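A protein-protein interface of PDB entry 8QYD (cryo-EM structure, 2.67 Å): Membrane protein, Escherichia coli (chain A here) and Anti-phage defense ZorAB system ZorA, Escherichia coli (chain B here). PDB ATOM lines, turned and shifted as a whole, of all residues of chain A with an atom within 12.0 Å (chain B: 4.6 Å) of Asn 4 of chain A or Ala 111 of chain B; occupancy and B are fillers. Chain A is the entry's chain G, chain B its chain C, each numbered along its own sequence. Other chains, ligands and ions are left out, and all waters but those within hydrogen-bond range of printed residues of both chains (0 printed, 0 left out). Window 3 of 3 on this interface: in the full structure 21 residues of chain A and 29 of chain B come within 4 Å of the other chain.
OG of Ser 115 of chain B lies within hydrogen-bond range of ND2 of Asn 4 of chain A (3.2 Å).
The side-chain amide oxygen of Asn 4 of chain A is in hydrogen-bond range of the backbone NH of Phe 6 of chain A, at 3.0 Å.
The side-chain amide nitrogen of Asn 4 of chain A lies close to the backbone NH of Gly 7 of chain A, at 3.0 Å.
The backbone carbonyl oxygen (O) of Gly 7 of chain A is in hydrogen-bond range of the side-chain amino group (NZ) of Lys 9 of chain A.
Asn 4 of chain A touches Ala 111 of chain B.
Pro 112 of chain B touches Asn 4 of chain A.
CB of Ser 115 of chain B touches O of Phe 6 of chain A (3.6 Å).
Phe 6 of chain A touches Phe 116 of chain B.
Ser 115 of chain B touches Gly 7 of chain A (OG to CA, 3.6 Å).
Ser 115 of chain B touches Val 8 of chain A (O to CG2, 3.4 Å).
Gly 3 of chain A touches none of the printed residues of chain B.
Of chain B, only Ala 111, Pro 112 and Ser 115 come within 4 Å of Asn 4 of chain A.
Printed residues of chain B within 4 Å of Phe 6 of chain A: Ser 115 (3.6 Å) and Phe 116 (3.97 Å).
Of the printed residues of chain B, Gly 7 of chain A touches Ser 115 (3.6 Å).
Of the printed residues of chain B, Val 8 of chain A touches Ser 115 (3.4 Å).
No residue of chain A comes within 4 Å of Phe 87 of chain B.
No residue of chain A comes within 4 Å of Thr 110 of chain B.
Of chain A, only Asn 4 (3.3 Å) comes within 4 Å of Ala 111 of chain B.
Pro 112 of chain B touches just one residue of chain A: Asn 4 (3.4 Å).
No residue of chain A comes within 4 Å of Ser 113 of chain B.
Ser 115 of chain B touches just these residues of chain A: Asn 4, Phe 6, Gly 7 and Val 8.
Printed residues of chain A within 4 Å of Phe 116 of chain B: Phe 6 (3.97 Å).
The nearest residue of chain B that does not touch Asn 4 of chain A is Thr 110 of chain B (4.1 Å).
The nearest residue of chain A that does not touch Ala 111 of chain B is Phe 6 of chain A (5.2 Å).
Hydrophobic or aromatic side chains of chain A that line the printed part of chain B: Phe 6 and Val 8.
Of the 9 printed residues of chain B, 4 touch a printed residue of chain A.
Among the printed residues, no Asp or Glu carboxylate lies within 4 Å of a Lys or Arg side-chain nitrogen of the other chain.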
ATOM      1  N   MET A   1      18.516   6.672  -7.198  1.00  0.00           N
ATOM      2  CA  MET A   1      19.379   5.900  -6.312  1.00  0.00           C
ATOM      3  C   MET A   1      20.467   5.169  -7.086  1.00  0.00           C
ATOM      4  O   MET A   1      21.592   5.030  -6.608  1.00  0.00           O
ATOM      5  CB  MET A   1      18.552   4.906  -5.494  1.00  0.00           C
ATOM      6  CG  MET A   1      19.354   4.135  -4.459  1.00  0.00           C
ATOM      7  SD  MET A   1      20.058   5.198  -3.189  1.00  0.00           S
ATOM      8  CE  MET A   1      18.595   5.631  -2.263  1.00  0.00           C
ATOM      9  N   PHE A   2      20.130   4.707  -8.288  1.00  0.00           N
ATOM     10  CA  PHE A   2      21.080   3.944  -9.087  1.00  0.00           C
ATOM     11  C   PHE A   2      21.231   4.545 -10.476  1.00  0.00           C
ATOM     12  O   PHE A   2      21.225   3.824 -11.479  1.00  0.00           O
ATOM     13  CB  PHE A   2      20.643   2.482  -9.166  1.00  0.00           C
ATOM     14  CG  PHE A   2      20.845   1.733  -7.887  1.00  0.00           C
ATOM     15  CD1 PHE A   2      22.102   1.296  -7.518  1.00  0.00           C
ATOM     16  CD2 PHE A   2      19.786   1.500  -7.030  1.00  0.00           C
ATOM     17  CE1 PHE A   2      22.294   0.622  -6.335  1.00  0.00           C
ATOM     18  CE2 PHE A   2      19.972   0.825  -5.847  1.00  0.00           C
ATOM     19  CZ  PHE A   2      21.228   0.386  -5.497  1.00  0.00           C
ATOM     20  N   GLY A   3      21.366   5.868 -10.542  1.00  0.00           N
ATOM     21  CA  GLY A   3      21.569   6.523 -11.813  1.00  0.00           C
ATOM     22  C   GLY A   3      22.961   6.292 -12.364  1.00  0.00           C
ATOM     23  O   GLY A   3      23.902   5.945 -11.651  1.00  0.00           O
ATOM     24  N   ASN A   4      23.087   6.492 -13.672  1.00  0.00           N
ATOM     25  CA  ASN A   4      24.352   6.303 -14.370  1.00  0.00           C
ATOM     26  C   ASN A   4      25.081   7.640 -14.432  1.00  0.00           C
ATOM     27  O   ASN A   4      24.598   8.592 -15.055  1.00  0.00           O
ATOM     28  CB  ASN A   4      24.112   5.737 -15.767  1.00  0.00           C
ATOM     29  CG  ASN A   4      25.365   5.729 -16.616  1.00  0.00           C
ATOM     30  OD1 ASN A   4      26.456   5.431 -16.130  1.00  0.00           O
ATOM     31  ND2 ASN A   4      25.215   6.053 -17.894  1.00  0.00           N
ATOM     32  N   ALA A   5      26.243   7.714 -13.781  1.00  0.00           N
ATOM     33  CA  ALA A   5      27.026   8.941 -13.798  1.00  0.00           C
ATOM     34  C   ALA A   5      27.724   9.165 -15.131  1.00  0.00           C
ATOM     35  O   ALA A   5      28.131  10.293 -15.421  1.00  0.00           O
ATOM     36  CB  ALA A   5      28.061   8.925 -12.673  1.00  0.00           C
ATOM     37  N   PHE A   6      27.859   8.124 -15.946  1.00  0.00           N
ATOM     38  CA  PHE A   6      28.612   8.201 -17.187  1.00  0.00           C
ATOM     39  C   PHE A   6      27.749   8.536 -18.394  1.00  0.00           C
ATOM     40  O   PHE A   6      28.260   8.531 -19.519  1.00  0.00           O
ATOM     41  CB  PHE A   6      29.360   6.886 -17.424  1.00  0.00           C
ATOM     42  CG  PHE A   6      30.472   6.650 -16.450  1.00  0.00           C
ATOM     43  CD1 PHE A   6      30.228   6.039 -15.235  1.00  0.00           C
ATOM     44  CD2 PHE A   6      31.757   7.068 -16.735  1.00  0.00           C
ATOM     45  CE1 PHE A   6      31.247   5.835 -14.333  1.00  0.00           C
ATOM     46  CE2 PHE A   6      32.780   6.865 -15.836  1.00  0.00           C
ATOM     47  CZ  PHE A   6      32.524   6.250 -14.634  1.00  0.00           C
ATOM     48  N   GLY A   7      26.464   8.815 -18.197  1.00  0.00           N
ATOM     49  CA  GLY A   7      25.631   9.279 -19.288  1.00  0.00           C
ATOM     50  C   GLY A   7      26.133  10.596 -19.846  1.00  0.00           C
ATOM     51  O   GLY A   7      26.260  11.580 -19.112  1.00  0.00           O
ATOM     52  N   VAL A   8      26.424  10.627 -21.141  1.00  0.00           N
ATOM     53  CA  VAL A   8      27.020  11.795 -21.777  1.00  0.00           C
ATOM     54  C   VAL A   8      25.944  12.580 -22.510  1.00  0.00           C
ATOM     55  O   VAL A   8      24.912  12.036 -22.923  1.00  0.00           O
ATOM     56  CB  VAL A   8      28.160  11.388 -22.735  1.00  0.00           C
ATOM     57  CG1 VAL A   8      29.380  10.950 -21.944  1.00  0.00           C
ATOM     58  CG2 VAL A   8      27.698  10.279 -23.668  1.00  0.00           C
ATOM     59  N   LYS A   9      26.185  13.879 -22.665  1.00  0.00           N
ATOM     60  CA  LYS A   9      25.280  14.778 -23.363  1.00  0.00           C
ATOM     61  C   LYS A   9      26.016  15.432 -24.524  1.00  0.00           C
ATOM     62  O   LYS A   9      27.204  15.752 -24.415  1.00  0.00           O
ATOM     63  CB  LYS A   9      24.723  15.857 -22.423  1.00  0.00           C
ATOM     64  CG  LYS A   9      23.527  15.421 -21.580  1.00  0.00           C
ATOM     65  CD  LYS A   9      23.940  14.489 -20.449  1.00  0.00           C
ATOM     66  CE  LYS A   9      24.752  15.228 -19.396  1.00  0.00           C
ATOM     67  NZ  LYS A   9      25.117  14.351 -18.248  1.00  0.00           N
ATOM     68  N   PHE B  87      33.024   0.717 -21.697  1.00  0.00           N
ATOM     69  CA  PHE B  87      31.783  -0.036 -21.561  1.00  0.00           C
ATOM     70  C   PHE B  87      31.992  -1.305 -20.744  1.00  0.00           C
ATOM     71  O   PHE B  87      31.181  -1.628 -19.871  1.00  0.00           O
ATOM     72  CB  PHE B  87      31.228  -0.370 -22.944  1.00  0.00           C
ATOM     73  CG  PHE B  87      29.978  -1.191 -22.914  1.00  0.00           C
ATOM     74  CD1 PHE B  87      28.829  -0.707 -22.322  1.00  0.00           C
ATOM     75  CD2 PHE B  87      29.950  -2.448 -23.485  1.00  0.00           C
ATOM     76  CE1 PHE B  87      27.681  -1.463 -22.295  1.00  0.00           C
ATOM     77  CE2 PHE B  87      28.805  -3.207 -23.461  1.00  0.00           C
ATOM     78  CZ  PHE B  87      27.669  -2.714 -22.868  1.00  0.00           C
ATOM     79  N   SER B  90      32.249  -0.640 -17.245  1.00  0.00           N
ATOM     80  CA  SER B  90      30.916  -0.340 -16.737  1.00  0.00           C
ATOM     81  C   SER B  90      30.049  -1.583 -16.569  1.00  0.00           C
ATOM     82  O   SER B  90      29.010  -1.506 -15.907  1.00  0.00           O
ATOM     83  CB  SER B  90      30.198   0.640 -17.661  1.00  0.00           C
ATOM     84  OG  SER B  90      29.508  -0.055 -18.680  1.00  0.00           O
ATOM     85  N   ALA B 109      24.457  -4.931 -17.047  1.00  0.00           N
ATOM     86  CA  ALA B 109      24.696  -3.605 -17.592  1.00  0.00           C
ATOM     87  C   ALA B 109      24.285  -2.566 -16.560  1.00  0.00           C
ATOM     88  O   ALA B 109      23.118  -2.511 -16.162  1.00  0.00           O
ATOM     89  CB  ALA B 109      23.925  -3.404 -18.894  1.00  0.00           C
ATOM     90  N   THR B 110      25.240  -1.752 -16.126  1.00  0.00           N
ATOM     91  CA  THR B 110      24.967  -0.661 -15.203  1.00  0.00           C
ATOM     92  C   THR B 110      24.884   0.689 -15.897  1.00  0.00           C
ATOM     93  O   THR B 110      24.713   1.708 -15.223  1.00  0.00           O
ATOM     94  CB  THR B 110      26.035  -0.614 -14.110  1.00  0.00           C
ATOM     95  OG1 THR B 110      27.324  -0.434 -14.707  1.00  0.00           O
ATOM     96  CG2 THR B 110      26.032  -1.908 -13.319  1.00  0.00           C
ATOM     97  N   ALA B 111      24.997   0.720 -17.222  1.00  0.00           N
ATOM     98  CA  ALA B 111      24.929   1.956 -17.987  1.00  0.00           C
ATOM     99  C   ALA B 111      24.517   1.614 -19.405  1.00  0.00           C
ATOM    100  O   ALA B 111      24.770   0.495 -19.863  1.00  0.00           O
ATOM    101  CB  ALA B 111      26.279   2.686 -17.986  1.00  0.00           C
ATOM    102  N   PRO B 112      23.882   2.539 -20.122  1.00  0.00           N
ATOM    103  CA  PRO B 112      23.584   2.292 -21.534  1.00  0.00           C
ATOM    104  C   PRO B 112      24.861   2.171 -22.349  1.00  0.00           C
ATOM    105  O   PRO B 112      25.891   2.759 -22.024  1.00  0.00           O
ATOM    106  CB  PRO B 112      22.771   3.522 -21.949  1.00  0.00           C
ATOM    107  CG  PRO B 112      22.263   4.094 -20.678  1.00  0.00           C
ATOM    108  CD  PRO B 112      23.308   3.811 -19.655  1.00  0.00           C
ATOM    109  N   SER B 113      24.783   1.385 -23.422  1.00  0.00           N
ATOM    110  CA  SER B 113      25.940   1.229 -24.294  1.00  0.00           C
ATOM    111  C   SER B 113      26.250   2.515 -25.046  1.00  0.00           C
ATOM    112  O   SER B 113      27.409   2.762 -25.394  1.00  0.00           O
ATOM    113  CB  SER B 113      25.706   0.086 -25.274  1.00  0.00           C
ATOM    114  OG  SER B 113      26.865  -0.143 -26.045  1.00  0.00           O
ATOM    115  N   SER B 115      26.353   5.382 -23.864  1.00  0.00           N
ATOM    116  CA  SER B 115      27.129   6.294 -23.034  1.00  0.00           C
ATOM    117  C   SER B 115      28.596   6.303 -23.433  1.00  0.00           C
ATOM    118  O   SER B 115      29.300   7.287 -23.186  1.00  0.00           O
ATOM    119  CB  SER B 115      26.987   5.912 -21.564  1.00  0.00           C
ATOM    120  OG  SER B 115      25.679   6.171 -21.095  1.00  0.00           O
ATOM    121  N   PHE B 116      29.070   5.227 -24.040  1.00  0.00           N
ATOM    122  CA  PHE B 116      30.465   5.086 -24.429  1.00  0.00           C
ATOM    123  C   PHE B 116      30.653   4.993 -25.932  1.00  0.00           C
ATOM    124  O   PHE B 116      31.607   5.563 -26.465  1.00  0.00           O
ATOM    125  CB  PHE B 116      31.061   3.853 -23.744  1.00  0.00           C
ATOM    126  CG  PHE B 116      30.708   3.751 -22.288  1.00  0.00           C
ATOM    127  CD1 PHE B 116      31.388   4.501 -21.348  1.00  0.00           C
ATOM    128  CD2 PHE B 116      29.688   2.919 -21.862  1.00  0.00           C
ATOM    129  CE1 PHE B 116      31.068   4.418 -20.015  1.00  0.00           C
ATOM    130  CE2 PHE B 116      29.363   2.835 -20.527  1.00  0.00           C
ATOM    131  CZ  PHE B 116      30.053   3.585 -19.604  1.00  0.00           C
